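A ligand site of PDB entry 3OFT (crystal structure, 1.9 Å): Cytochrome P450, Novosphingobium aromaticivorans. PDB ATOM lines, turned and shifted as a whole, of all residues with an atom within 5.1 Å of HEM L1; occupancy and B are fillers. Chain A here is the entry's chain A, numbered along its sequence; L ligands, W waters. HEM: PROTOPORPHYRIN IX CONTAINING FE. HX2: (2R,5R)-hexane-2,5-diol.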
ATOM      1  N   TRP A  61      10.975 -36.706  -9.259  1.00  0.00           N
ATOM      2  CA  TRP A  61      10.510 -35.335  -8.995  1.00  0.00           C
ATOM      3  C   TRP A  61      11.700 -34.453  -8.616  1.00  0.00           C
ATOM      4  O   TRP A  61      11.744 -33.261  -8.944  1.00  0.00           O
ATOM      5  CB  TRP A  61       9.497 -35.354  -7.851  1.00  0.00           C
ATOM      6  CG  TRP A  61       8.554 -34.170  -7.789  1.00  0.00           C
ATOM      7  CD1 TRP A  61       8.858 -32.843  -7.844  1.00  0.00           C
ATOM      8  CD2 TRP A  61       7.155 -34.246  -7.569  1.00  0.00           C
ATOM      9  NE1 TRP A  61       7.689 -32.078  -7.707  1.00  0.00           N
ATOM     10  CE2 TRP A  61       6.645 -32.929  -7.533  1.00  0.00           C
ATOM     11  CE3 TRP A  61       6.265 -35.315  -7.412  1.00  0.00           C
ATOM     12  CZ2 TRP A  61       5.270 -32.659  -7.355  1.00  0.00           C
ATOM     13  CZ3 TRP A  61       4.907 -35.051  -7.221  1.00  0.00           C
ATOM     14  CH2 TRP A  61       4.425 -33.723  -7.194  1.00  0.00           C
ATOM     15  N   SER A  69      11.160 -29.047 -16.275  1.00  0.00           N
ATOM     16  CA  SER A  69       9.845 -28.535 -15.870  1.00  0.00           C
ATOM     17  C   SER A  69       9.221 -27.734 -16.993  1.00  0.00           C
ATOM     18  O   SER A  69       8.151 -27.136 -16.819  1.00  0.00           O
ATOM     19  CB  SER A  69       9.950 -27.656 -14.630  1.00  0.00           C
ATOM     20  OG  SER A  69      10.231 -28.469 -13.493  1.00  0.00           O
ATOM     21  N   ILE A  85       6.566 -18.380 -14.351  1.00  0.00           N
ATOM     22  CA  ILE A  85       7.819 -18.170 -13.631  1.00  0.00           C
ATOM     23  C   ILE A  85       7.545 -18.217 -12.108  1.00  0.00           C
ATOM     24  O   ILE A  85       6.651 -17.525 -11.603  1.00  0.00           O
ATOM     25  CB  ILE A  85       8.442 -16.789 -13.974  1.00  0.00           C
ATOM     26  CG1 ILE A  85       9.052 -16.808 -15.386  1.00  0.00           C
ATOM     27  CG2 ILE A  85       9.534 -16.415 -12.941  1.00  0.00           C
ATOM     28  CD1 ILE A  85       9.527 -15.354 -15.786  1.00  0.00           C
ATOM     29  N   PRO A  86       8.322 -19.028 -11.357  1.00  0.00           N
ATOM     30  CA  PRO A  86       9.451 -19.878 -11.688  1.00  0.00           C
ATOM     31  C   PRO A  86       9.051 -21.310 -12.131  1.00  0.00           C
ATOM     32  O   PRO A  86       9.944 -22.090 -12.447  1.00  0.00           O
ATOM     33  CB  PRO A  86      10.252 -19.934 -10.381  1.00  0.00           C
ATOM     34  CG  PRO A  86       9.289 -19.588  -9.319  1.00  0.00           C
ATOM     35  CD  PRO A  86       8.045 -19.031  -9.909  1.00  0.00           C
ATOM     36  N   LEU A  87       7.749 -21.640 -12.180  1.00  0.00           N
ATOM     37  CA  LEU A  87       7.316 -23.071 -12.227  1.00  0.00           C
ATOM     38  C   LEU A  87       7.941 -23.835 -13.393  1.00  0.00           C
ATOM     39  O   LEU A  87       8.267 -25.024 -13.267  1.00  0.00           O
ATOM     40  CB  LEU A  87       5.783 -23.204 -12.264  1.00  0.00           C
ATOM     41  CG  LEU A  87       5.157 -24.616 -12.276  1.00  0.00           C
ATOM     42  CD1 LEU A  87       5.445 -25.393 -10.946  1.00  0.00           C
ATOM     43  CD2 LEU A  87       3.669 -24.495 -12.512  1.00  0.00           C
ATOM     44  N   HIS A  94      16.052 -20.659 -13.350  1.00  0.00           N
ATOM     45  CA  HIS A  94      15.074 -20.973 -12.321  1.00  0.00           C
ATOM     46  C   HIS A  94      15.529 -20.414 -10.958  1.00  0.00           C
ATOM     47  O   HIS A  94      14.805 -19.730 -10.269  1.00  0.00           O
ATOM     48  CB  HIS A  94      14.830 -22.497 -12.222  1.00  0.00           C
ATOM     49  CG  HIS A  94      14.131 -22.884 -10.966  1.00  0.00           C
ATOM     50  ND1 HIS A  94      12.821 -22.538 -10.711  1.00  0.00           N
ATOM     51  CD2 HIS A  94      14.586 -23.504  -9.866  1.00  0.00           C
ATOM     52  CE1 HIS A  94      12.481 -22.985  -9.512  1.00  0.00           C
ATOM     53  NE2 HIS A  94      13.548 -23.571  -8.978  1.00  0.00           N
ATOM     54  N   ARG A  98      13.446 -17.741  -8.790  1.00  0.00           N
ATOM     55  CA  ARG A  98      12.889 -18.285  -7.548  1.00  0.00           C
ATOM     56  C   ARG A  98      13.345 -17.452  -6.334  1.00  0.00           C
ATOM     57  O   ARG A  98      12.570 -17.196  -5.422  1.00  0.00           O
ATOM     58  CB  ARG A  98      13.307 -19.730  -7.332  1.00  0.00           C
ATOM     59  CG  ARG A  98      12.637 -20.404  -6.106  1.00  0.00           C
ATOM     60  CD  ARG A  98      13.088 -21.851  -5.964  1.00  0.00           C
ATOM     61  NE  ARG A  98      12.789 -22.353  -4.630  1.00  0.00           N
ATOM     62  CZ  ARG A  98      11.708 -23.051  -4.283  1.00  0.00           C
ATOM     63  NH1 ARG A  98      11.621 -23.473  -3.006  1.00  0.00           N
ATOM     64  NH2 ARG A  98      10.752 -23.371  -5.153  1.00  0.00           N
ATOM     65  N   VAL A 101      11.169 -14.495  -5.487  1.00  0.00           N
ATOM     66  CA  VAL A 101       9.795 -14.948  -5.165  1.00  0.00           C
ATOM     67  C   VAL A 101       9.747 -15.563  -3.742  1.00  0.00           C
ATOM     68  O   VAL A 101       8.837 -15.259  -2.983  1.00  0.00           O
ATOM     69  CB  VAL A 101       9.317 -15.989  -6.199  1.00  0.00           C
ATOM     70  CG1 VAL A 101       8.020 -16.657  -5.743  1.00  0.00           C
ATOM     71  CG2 VAL A 101       9.142 -15.303  -7.576  1.00  0.00           C
ATOM     72  N   LEU A 105       7.692 -14.552  -0.035  1.00  0.00           N
ATOM     73  CA  LEU A 105       6.888 -15.503   0.720  1.00  0.00           C
ATOM     74  C   LEU A 105       7.507 -16.098   1.996  1.00  0.00           C
ATOM     75  O   LEU A 105       7.026 -17.125   2.510  1.00  0.00           O
ATOM     76  CB  LEU A 105       6.460 -16.633  -0.205  1.00  0.00           C
ATOM     77  CG  LEU A 105       5.407 -16.160  -1.210  1.00  0.00           C
ATOM     78  CD1 LEU A 105       5.346 -17.096  -2.454  1.00  0.00           C
ATOM     79  CD2 LEU A 105       4.029 -16.003  -0.506  1.00  0.00           C
ATOM     80  N   LEU A 152      -3.349 -10.623   0.026  1.00  0.00           N
ATOM     81  CA  LEU A 152      -1.887 -10.710  -0.164  1.00  0.00           C
ATOM     82  C   LEU A 152      -1.298  -9.558  -0.995  1.00  0.00           C
ATOM     83  O   LEU A 152      -0.204  -9.085  -0.688  1.00  0.00           O
ATOM     84  CB  LEU A 152      -1.444 -12.018  -0.844  1.00  0.00           C
ATOM     85  CG  LEU A 152      -1.821 -13.414  -0.319  1.00  0.00           C
ATOM     86  CD1 LEU A 152      -1.381 -14.563  -1.290  1.00  0.00           C
ATOM     87  CD2 LEU A 152      -1.318 -13.670   1.090  1.00  0.00           C
ATOM     88  N   LEU A 205       2.697  -8.529  -1.188  1.00  0.00           N
ATOM     89  CA  LEU A 205       3.421  -9.599  -1.882  1.00  0.00           C
ATOM     90  C   LEU A 205       4.005  -9.217  -3.225  1.00  0.00           C
ATOM     91  O   LEU A 205       5.189  -9.482  -3.463  1.00  0.00           O
ATOM     92  CB  LEU A 205       2.541 -10.832  -2.061  1.00  0.00           C
ATOM     93  CG  LEU A 205       3.127 -12.091  -2.710  1.00  0.00           C
ATOM     94  CD1 LEU A 205       4.441 -12.556  -2.029  1.00  0.00           C
ATOM     95  CD2 LEU A 205       2.062 -13.244  -2.778  1.00  0.00           C
ATOM     96  N   ASN A 230       1.804 -17.009 -12.349  1.00  0.00           N
ATOM     97  CA  ASN A 230       2.133 -18.162 -11.499  1.00  0.00           C
ATOM     98  C   ASN A 230       1.671 -18.035 -10.038  1.00  0.00           C
ATOM     99  O   ASN A 230       1.153 -19.019  -9.480  1.00  0.00           O
ATOM    100  CB  ASN A 230       3.624 -18.459 -11.589  1.00  0.00           C
ATOM    101  CG  ASN A 230       3.990 -19.872 -11.143  1.00  0.00           C
ATOM    102  OD1 ASN A 230       3.192 -20.654 -10.609  1.00  0.00           O
ATOM    103  ND2 ASN A 230       5.213 -20.183 -11.346  1.00  0.00           N
ATOM    104  N   LEU A 231       1.863 -16.875  -9.420  1.00  0.00           N
ATOM    105  CA  LEU A 231       1.408 -16.664  -8.037  1.00  0.00           C
ATOM    106  C   LEU A 231      -0.103 -16.760  -7.922  1.00  0.00           C
ATOM    107  O   LEU A 231      -0.612 -17.433  -6.999  1.00  0.00           O
ATOM    108  CB  LEU A 231       1.912 -15.334  -7.492  1.00  0.00           C
ATOM    109  CG  LEU A 231       3.403 -15.315  -7.164  1.00  0.00           C
ATOM    110  CD1 LEU A 231       3.631 -13.907  -6.617  1.00  0.00           C
ATOM    111  CD2 LEU A 231       3.801 -16.359  -6.101  1.00  0.00           C
ATOM    112  N   GLY A 234      -1.064 -20.527  -8.892  1.00  0.00           N
ATOM    113  CA  GLY A 234      -0.425 -21.503  -7.996  1.00  0.00           C
ATOM    114  C   GLY A 234      -1.109 -21.639  -6.638  1.00  0.00           C
ATOM    115  O   GLY A 234      -1.033 -22.672  -6.001  1.00  0.00           O
ATOM    116  N   GLY A 235      -1.800 -20.576  -6.215  1.00  0.00           N
ATOM    117  CA  GLY A 235      -2.446 -20.533  -4.905  1.00  0.00           C
ATOM    118  C   GLY A 235      -3.972 -20.675  -4.949  1.00  0.00           C
ATOM    119  O   GLY A 235      -4.616 -20.688  -3.912  1.00  0.00           O
ATOM    120  N   THR A 238      -5.075 -25.178  -5.828  1.00  0.00           N
ATOM    121  CA  THR A 238      -4.402 -26.054  -4.822  1.00  0.00           C
ATOM    122  C   THR A 238      -4.980 -25.815  -3.419  1.00  0.00           C
ATOM    123  O   THR A 238      -5.268 -26.779  -2.685  1.00  0.00           O
ATOM    124  CB  THR A 238      -2.904 -25.739  -4.753  1.00  0.00           C
ATOM    125  OG1 THR A 238      -2.761 -24.308  -4.643  1.00  0.00           O
ATOM    126  CG2 THR A 238      -2.165 -26.255  -6.013  1.00  0.00           C
ATOM    127  N   VAL A 239      -5.161 -24.541  -3.065  1.00  0.00           N
ATOM    128  CA  VAL A 239      -5.671 -24.180  -1.744  1.00  0.00           C
ATOM    129  C   VAL A 239      -7.157 -24.556  -1.644  1.00  0.00           C
ATOM    130  O   VAL A 239      -7.572 -25.134  -0.650  1.00  0.00           O
ATOM    131  CB  VAL A 239      -5.409 -22.715  -1.365  1.00  0.00           C
ATOM    132  CG1 VAL A 239      -6.101 -22.329  -0.033  1.00  0.00           C
ATOM    133  CG2 VAL A 239      -3.870 -22.502  -1.211  1.00  0.00           C
ATOM    134  N   MET A 242      -7.198 -28.389  -1.065  1.00  0.00           N
ATOM    135  CA  MET A 242      -6.736 -28.796   0.266  1.00  0.00           C
ATOM    136  C   MET A 242      -7.784 -28.444   1.334  1.00  0.00           C
ATOM    137  O   MET A 242      -8.059 -29.258   2.230  1.00  0.00           O
ATOM    138  CB  MET A 242      -5.375 -28.177   0.592  1.00  0.00           C
ATOM    139  CG  MET A 242      -4.759 -28.695   1.965  1.00  0.00           C
ATOM    140  SD  MET A 242      -4.611 -30.499   2.135  1.00  0.00           S
ATOM    141  CE  MET A 242      -3.208 -30.784   1.008  1.00  0.00           C
ATOM    142  N   MET A 275      -2.430 -32.317   5.654  1.00  0.00           N
ATOM    143  CA  MET A 275      -1.748 -31.966   4.381  1.00  0.00           C
ATOM    144  C   MET A 275      -0.949 -33.146   3.823  1.00  0.00           C
ATOM    145  O   MET A 275      -0.919 -33.378   2.615  1.00  0.00           O
ATOM    146  CB  MET A 275      -0.907 -30.700   4.498  1.00  0.00           C
ATOM    147  CG  MET A 275      -1.784 -29.470   4.809  1.00  0.00           C
ATOM    148  SD  MET A 275      -0.929 -27.920   5.200  1.00  0.00           S
ATOM    149  CE  MET A 275      -0.381 -27.478   3.559  1.00  0.00           C
ATOM    150  N   VAL A 281      -1.933 -33.087  -5.761  1.00  0.00           N
ATOM    151  CA  VAL A 281      -1.196 -32.422  -6.837  1.00  0.00           C
ATOM    152  C   VAL A 281      -0.341 -33.424  -7.625  1.00  0.00           C
ATOM    153  O   VAL A 281       0.328 -34.265  -7.020  1.00  0.00           O
ATOM    154  CB  VAL A 281      -0.404 -31.142  -6.360  1.00  0.00           C
ATOM    155  CG1 VAL A 281       0.300 -30.530  -7.565  1.00  0.00           C
ATOM    156  CG2 VAL A 281      -1.404 -30.067  -5.770  1.00  0.00           C
ATOM    157  N   VAL A 283       2.395 -33.529 -11.184  1.00  0.00           N
ATOM    158  CA  VAL A 283       3.145 -32.654 -12.091  1.00  0.00           C
ATOM    159  C   VAL A 283       3.691 -33.411 -13.287  1.00  0.00           C
ATOM    160  O   VAL A 283       3.842 -34.655 -13.238  1.00  0.00           O
ATOM    161  CB  VAL A 283       4.322 -31.941 -11.384  1.00  0.00           C
ATOM    162  CG1 VAL A 283       3.809 -31.059 -10.229  1.00  0.00           C
ATOM    163  CG2 VAL A 283       5.421 -32.967 -10.933  1.00  0.00           C
ATOM    164  N   ARG A 285       6.917 -33.725 -16.301  1.00  0.00           N
ATOM    165  CA  ARG A 285       8.295 -33.332 -16.668  1.00  0.00           C
ATOM    166  C   ARG A 285       8.567 -33.826 -18.065  1.00  0.00           C
ATOM    167  O   ARG A 285       7.954 -34.795 -18.483  1.00  0.00           O
ATOM    168  CB  ARG A 285       9.321 -34.041 -15.743  1.00  0.00           C
ATOM    169  CG  ARG A 285       9.206 -33.683 -14.224  1.00  0.00           C
ATOM    170  CD  ARG A 285       9.584 -32.218 -14.024  1.00  0.00           C
ATOM    171  NE  ARG A 285       9.740 -31.883 -12.589  1.00  0.00           N
ATOM    172  CZ  ARG A 285       8.881 -31.153 -11.904  1.00  0.00           C
ATOM    173  NH1 ARG A 285       7.764 -30.657 -12.434  1.00  0.00           N
ATOM    174  NH2 ARG A 285       9.183 -30.877 -10.636  1.00  0.00           N
ATOM    175  N   THR A 336       5.637 -35.342  -0.027  1.00  0.00           N
ATOM    176  CA  THR A 336       5.652 -34.766  -1.379  1.00  0.00           C
ATOM    177  C   THR A 336       4.443 -33.892  -1.669  1.00  0.00           C
ATOM    178  O   THR A 336       4.225 -33.509  -2.821  1.00  0.00           O
ATOM    179  CB  THR A 336       5.933 -35.902  -2.411  1.00  0.00           C
ATOM    180  OG1 THR A 336       7.191 -36.515  -2.065  1.00  0.00           O
ATOM    181  CG2 THR A 336       6.074 -35.382  -3.828  1.00  0.00           C
ATOM    182  N   THR A 337       3.649 -33.521  -0.642  1.00  0.00           N
ATOM    183  CA  THR A 337       2.463 -32.678  -0.907  1.00  0.00           C
ATOM    184  C   THR A 337       2.857 -31.387  -1.648  1.00  0.00           C
ATOM    185  O   THR A 337       2.153 -30.958  -2.585  1.00  0.00           O
ATOM    186  CB  THR A 337       1.675 -32.321   0.378  1.00  0.00           C
ATOM    187  OG1 THR A 337       1.220 -33.549   0.961  1.00  0.00           O
ATOM    188  CG2 THR A 337       0.451 -31.429   0.031  1.00  0.00           C
ATOM    189  N   MET A 338       3.992 -30.804  -1.266  1.00  0.00           N
ATOM    190  CA  MET A 338       4.449 -29.554  -1.819  1.00  0.00           C
ATOM    191  C   MET A 338       5.566 -29.761  -2.870  1.00  0.00           C
ATOM    192  O   MET A 338       6.168 -28.809  -3.315  1.00  0.00           O
ATOM    193  CB  MET A 338       4.948 -28.673  -0.677  1.00  0.00           C
ATOM    194  CG  MET A 338       3.951 -28.543   0.488  1.00  0.00           C
ATOM    195  SD  MET A 338       2.370 -27.874  -0.014  1.00  0.00           S
ATOM    196  CE  MET A 338       2.904 -26.381  -0.670  1.00  0.00           C
ATOM    197  N   GLY A 339       5.778 -31.003  -3.274  1.00  0.00           N
ATOM    198  CA  GLY A 339       6.822 -31.329  -4.251  1.00  0.00           C
ATOM    199  C   GLY A 339       8.136 -31.675  -3.587  1.00  0.00           C
ATOM    200  O   GLY A 339       8.187 -32.003  -2.387  1.00  0.00           O
ATOM    201  N   ALA A 342      14.341 -28.625  -5.997  1.00  0.00           N
ATOM    202  CA  ALA A 342      14.527 -27.206  -6.358  1.00  0.00           C
ATOM    203  C   ALA A 342      13.198 -26.456  -6.510  1.00  0.00           C
ATOM    204  O   ALA A 342      13.144 -25.307  -6.198  1.00  0.00           O
ATOM    205  CB  ALA A 342      15.286 -27.108  -7.649  1.00  0.00           C
ATOM    206  N   HIS A 343      12.152 -27.115  -7.017  1.00  0.00           N
ATOM    207  CA  HIS A 343      10.890 -26.442  -7.318  1.00  0.00           C
ATOM    208  C   HIS A 343       9.866 -26.532  -6.180  1.00  0.00           C
ATOM    209  O   HIS A 343       8.697 -26.139  -6.342  1.00  0.00           O
ATOM    210  CB  HIS A 343      10.269 -27.025  -8.613  1.00  0.00           C
ATOM    211  CG  HIS A 343      10.946 -26.588  -9.889  1.00  0.00           C
ATOM    212  ND1 HIS A 343      10.628 -25.421 -10.543  1.00  0.00           N
ATOM    213  CD2 HIS A 343      11.900 -27.201 -10.647  1.00  0.00           C
ATOM    214  CE1 HIS A 343      11.356 -25.307 -11.630  1.00  0.00           C
ATOM    215  NE2 HIS A 343      12.137 -26.380 -11.729  1.00  0.00           N
ATOM    216  N   ARG A 344      10.300 -27.033  -5.018  1.00  0.00           N
ATOM    217  CA  ARG A 344       9.328 -27.228  -3.894  1.00  0.00           C
ATOM    218  C   ARG A 344       8.514 -25.959  -3.633  1.00  0.00           C
ATOM    219  O   ARG A 344       9.057 -24.850  -3.560  1.00  0.00           O
ATOM    220  CB  ARG A 344      10.013 -27.744  -2.588  1.00  0.00           C
ATOM    221  CG  ARG A 344       8.976 -28.129  -1.475  1.00  0.00           C
ATOM    222  CD  ARG A 344       9.572 -28.924  -0.292  1.00  0.00           C
ATOM    223  NE  ARG A 344       8.505 -29.257   0.656  1.00  0.00           N
ATOM    224  CZ  ARG A 344       8.142 -28.475   1.674  1.00  0.00           C
ATOM    225  NH1 ARG A 344       8.814 -27.363   1.941  1.00  0.00           N
ATOM    226  NH2 ARG A 344       7.130 -28.836   2.449  1.00  0.00           N
ATOM    227  N   CYS A 345       7.190 -26.108  -3.471  1.00  0.00           N
ATOM    228  CA  CYS A 345       6.294 -24.937  -3.379  1.00  0.00           C
ATOM    229  C   CYS A 345       6.837 -23.766  -2.561  1.00  0.00           C
ATOM    230  O   CYS A 345       7.064 -23.917  -1.346  1.00  0.00           O
ATOM    231  CB  CYS A 345       4.945 -25.337  -2.750  1.00  0.00           C
ATOM    232  SG  CYS A 345       3.736 -24.104  -2.839  1.00  0.00           S
ATOM    233  N   VAL A 346       7.030 -22.602  -3.196  1.00  0.00           N
ATOM    234  CA  VAL A 346       7.369 -21.385  -2.465  1.00  0.00           C
ATOM    235  C   VAL A 346       6.264 -20.960  -1.518  1.00  0.00           C
ATOM    236  O   VAL A 346       6.515 -20.226  -0.577  1.00  0.00           O
ATOM    237  CB  VAL A 346       7.675 -20.162  -3.408  1.00  0.00           C
ATOM    238  CG1 VAL A 346       9.019 -20.383  -4.095  1.00  0.00           C
ATOM    239  CG2 VAL A 346       6.585 -19.960  -4.441  1.00  0.00           C
ATOM    240  N   GLY A 347       5.029 -21.359  -1.816  1.00  0.00           N
ATOM    241  CA  GLY A 347       3.918 -21.004  -0.913  1.00  0.00           C
ATOM    242  C   GLY A 347       3.677 -22.030   0.193  1.00  0.00           C
ATOM    243  O   GLY A 347       2.589 -22.012   0.776  1.00  0.00           O
ATOM    244  N   LEU A 350       2.938 -20.382   3.437  1.00  0.00           N
ATOM    245  CA  LEU A 350       1.649 -19.702   3.370  1.00  0.00           C
ATOM    246  C   LEU A 350       0.476 -20.676   3.366  1.00  0.00           C
ATOM    247  O   LEU A 350      -0.545 -20.411   4.047  1.00  0.00           O
ATOM    248  CB  LEU A 350       1.602 -18.783   2.151  1.00  0.00           C
ATOM    249  CG  LEU A 350       0.252 -18.148   1.797  1.00  0.00           C
ATOM    250  CD1 LEU A 350      -0.187 -17.213   2.924  1.00  0.00           C
ATOM    251  CD2 LEU A 350       0.357 -17.394   0.487  1.00  0.00           C
ATOM    252  N   ALA A 351       0.588 -21.760   2.601  1.00  0.00           N
ATOM    253  CA  ALA A 351      -0.486 -22.790   2.544  1.00  0.00           C
ATOM    254  C   ALA A 351      -0.737 -23.375   3.932  1.00  0.00           C
ATOM    255  O   ALA A 351      -1.879 -23.525   4.355  1.00  0.00           O
ATOM    256  CB  ALA A 351      -0.099 -23.938   1.552  1.00  0.00           C
ATOM    257  N   GLU A 354      -2.681 -20.888   5.905  1.00  0.00           N
ATOM    258  CA  GLU A 354      -4.082 -20.842   5.466  1.00  0.00           C
ATOM    259  C   GLU A 354      -4.887 -22.029   6.027  1.00  0.00           C
ATOM    260  O   GLU A 354      -6.039 -21.843   6.454  1.00  0.00           O
ATOM    261  CB  GLU A 354      -4.153 -20.868   3.948  1.00  0.00           C
ATOM    262  CG  GLU A 354      -3.579 -19.595   3.314  1.00  0.00           C
ATOM    263  CD  GLU A 354      -3.531 -19.696   1.763  1.00  0.00           C
ATOM    264  OE1 GLU A 354      -4.198 -18.937   1.082  1.00  0.00           O
ATOM    265  OE2 GLU A 354      -2.826 -20.566   1.214  1.00  0.00           O
HETATM  266  CHA HEM L   1       5.142 -25.117  -6.677  1.00  0.00           C
HETATM  267  CHB HEM L   1       1.667 -27.596  -4.338  1.00  0.00           C
HETATM  268  CHC HEM L   1      -0.007 -23.464  -2.493  1.00  0.00           C
HETATM  269  CHD HEM L   1       2.719 -20.993  -5.585  1.00  0.00           C
HETATM  270  C1A HEM L   1       4.378 -26.135  -6.134  1.00  0.00           C
HETATM  271  C2A HEM L   1       4.648 -27.541  -6.321  1.00  0.00           C
HETATM  272  C3A HEM L   1       3.716 -28.245  -5.687  1.00  0.00           C
HETATM  273  C4A HEM L   1       2.766 -27.301  -5.095  1.00  0.00           C
HETATM  274  CMA HEM L   1       3.639 -29.789  -5.683  1.00  0.00           C
HETATM  275  CAA HEM L   1       5.865 -28.138  -7.078  1.00  0.00           C
HETATM  276  CBA HEM L   1       5.539 -28.142  -8.553  1.00  0.00           C
HETATM  277  CGA HEM L   1       6.628 -28.810  -9.380  1.00  0.00           C
HETATM  278  O1A HEM L   1       6.523 -28.760 -10.649  1.00  0.00           O
HETATM  279  O2A HEM L   1       7.608 -29.409  -8.845  1.00  0.00           O
HETATM  280  C1B HEM L   1       0.901 -26.701  -3.604  1.00  0.00           C
HETATM  281  C2B HEM L   1      -0.158 -27.037  -2.684  1.00  0.00           C
HETATM  282  C3B HEM L   1      -0.605 -25.866  -2.174  1.00  0.00           C
HETATM  283  C4B HEM L   1       0.163 -24.789  -2.779  1.00  0.00           C
HETATM  284  CMB HEM L   1      -0.609 -28.476  -2.381  1.00  0.00           C
HETATM  285  CAB HEM L   1      -1.719 -25.559  -1.183  1.00  0.00           C
HETATM  286  CBB HEM L   1      -2.521 -26.508  -0.646  1.00  0.00           C
HETATM  287  C1C HEM L   1       0.555 -22.391  -3.120  1.00  0.00           C
HETATM  288  C2C HEM L   1       0.340 -20.979  -2.829  1.00  0.00           C
HETATM  289  C3C HEM L   1       1.097 -20.302  -3.738  1.00  0.00           C
HETATM  290  C4C HEM L   1       1.854 -21.255  -4.521  1.00  0.00           C
HETATM  291  CMC HEM L   1      -0.608 -20.439  -1.719  1.00  0.00           C
HETATM  292  CAC HEM L   1       1.325 -18.783  -3.923  1.00  0.00           C
HETATM  293  CBC HEM L   1       0.396 -17.881  -3.653  1.00  0.00           C
HETATM  294  C1D HEM L   1       3.624 -21.843  -6.126  1.00  0.00           C
HETATM  295  C2D HEM L   1       4.663 -21.439  -7.059  1.00  0.00           C
HETATM  296  C3D HEM L   1       5.431 -22.716  -7.349  1.00  0.00           C
HETATM  297  C4D HEM L   1       4.788 -23.776  -6.634  1.00  0.00           C
HETATM  298  CMD HEM L   1       4.972 -19.994  -7.583  1.00  0.00           C
HETATM  299  CAD HEM L   1       6.662 -22.795  -8.304  1.00  0.00           C
HETATM  300  CBD HEM L   1       7.894 -22.872  -7.385  1.00  0.00           C
HETATM  301  CGD HEM L   1       9.091 -23.145  -8.310  1.00  0.00           C
HETATM  302  O1D HEM L   1       8.929 -23.561  -9.471  1.00  0.00           O
HETATM  303  O2D HEM L   1      10.242 -22.998  -7.876  1.00  0.00           O
HETATM  304  NA  HEM L   1       3.218 -26.021  -5.360  1.00  0.00           N
HETATM  305  NB  HEM L   1       1.081 -25.330  -3.588  1.00  0.00           N
HETATM  306  NC  HEM L   1       1.513 -22.511  -4.126  1.00  0.00           N
HETATM  307  ND  HEM L   1       3.708 -23.212  -5.916  1.00  0.00           N
HETATM  308 FE   HEM L   1       2.427 -24.266  -4.691  1.00  0.00          FE
HETATM  309  C1  HX2 L   2       0.345 -27.826 -13.717  1.00  0.00           C
HETATM  310  O1  HX2 L   2       0.408 -30.166 -13.012  1.00  0.00           O
HETATM  311  C2  HX2 L   2       0.057 -28.831 -12.594  1.00  0.00           C
HETATM  312  O2  HX2 L   2       0.315 -25.476  -8.971  1.00  0.00           O
HETATM  313  C3  HX2 L   2       0.687 -28.454 -11.245  1.00  0.00           C
HETATM  314  C4  HX2 L   2       0.298 -27.034 -10.781  1.00  0.00           C
HETATM  315  C5  HX2 L   2       0.553 -26.843  -9.280  1.00  0.00           C
HETATM  316  C6  HX2 L   2       2.010 -27.182  -8.932  1.00  0.00           C
HETATM  317  O   HOH W   1       0.931 -24.240  -6.554  1.00  0.00           O
HETATM  318  O   HOH W   2       4.889 -28.154 -12.655  1.00  0.00           O
HETATM  319  O   HOH W   3       8.481 -27.285 -11.821  1.00  0.00           O
HETATM  320  O   HOH W   4       9.071 -29.605  -6.576  1.00  0.00           O
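The guanidinium group (NH2) of Arg 98 lies within salt-bridge range of an oxygen (O2D) of HEM L1, 2.8 Å away.
ND1 of His 343 sits at hydrogen-bond distance from O1D of HEM L1.
FE of HEM L1 is bound by SG of Cys 345 (2.3 Å).
The guanidinium group of Arg 285 lies within salt-bridge range of an oxygen (O2A) of HEM L1, at 2.8 Å.
NE1 of Trp 61 is in hydrogen-bond range of O2A of HEM L1 (2.9 Å).
A ring nitrogen (NE2) of His 94 lies within hydrogen-bond range of the backbone carbonyl oxygen (O) of Ala 342 (3.3 Å).
The backbone NH (N) of Leu 87 sits close to the side-chain amide nitrogen (ND2) of Asn 230, 3.0 Å away.
The backbone NH of Cys 345 sits at hydrogen-bond distance from the backbone carbonyl oxygen of Met 338.
The guanidinium group of Arg 98 is in hydrogen-bond range of the backbone carbonyl oxygen of Arg 344, at 2.8 Å.
The side-chain hydroxyl of Ser 69 is in hydrogen-bond range of a ring nitrogen (NE2) of His 343 (3.3 Å).
O of Gly 234 lies within hydrogen-bond range of OG1 of Thr 238 (2.7 Å).
NH2 of Arg 98 lies within hydrogen-bond range of O of Ala 342, at 3.2 Å.
The backbone carbonyl oxygen (O) of Ile 85 is in hydrogen-bond range of the side-chain amide nitrogen (ND2) of Asn 230 (3.0 Å).
O of Pro 86 sits close to O1D of HEM L1 (3.5 Å).
The backbone carbonyl oxygen (O) of Gly 234 sits close to a nitrogen (NC) of HEM L1 (3.2 Å).
Merely in contact with HEM L1: His 94 (2.8 Å), Leu 87 (3.2 Å), Met 338 (3.4 Å), Thr 238 (3.4 Å), Gly 339 (3.4 Å), Gly 235 (3.5 Å), Leu 231 (3.5 Å), Met 242 (3.5 Å), Val 346 (3.5 Å), Ala 351 (3.6 Å), Asn 230 (3.6 Å), Val 283 (3.6 Å), Thr 337 (3.6 Å), Glu 354 (3.7 Å), Val 239 (3.7 Å), Val 281 (3.8 Å) and Leu 350 (3.9 Å).
Hydrophobic or aromatic side chains within 4 Å of HEM L1: Trp 61, Pro 86, Leu 87, His 94, Val 239, Met 242, Val 281, Val 283, Met 338, His 343, Val 346, Leu 350 and Ala 351.
Of the 35 residues printed, 24 come within 4 Å of HEM L1.
The nearest printed residue that does not touch HEM L1 is Gly 347 (4.1 Å).
Water W1 lies within hydrogen-bond range of O of Gly 234 and O2 of HX2 L2.
Water W4 lies within hydrogen-bond range of an oxygen (O2A) of HEM L1 (2.7 Å), the indole nitrogen (NE1) of Trp 61 (3.1 Å), the backbone NH (N) of Arg 344 (3.2 Å) and the backbone carbonyl oxygen (O) of His 343 (3.5 Å).
Water W3 lies within hydrogen-bond range of the backbone carbonyl oxygen (O) of Leu 87 (2.7 Å), the side-chain hydroxyl (OG) of Ser 69 (2.7 Å), an oxygen (O1A) of HEM L1 (2.7 Å) and a ring nitrogen (ND1) of His 343 (3.1 Å).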
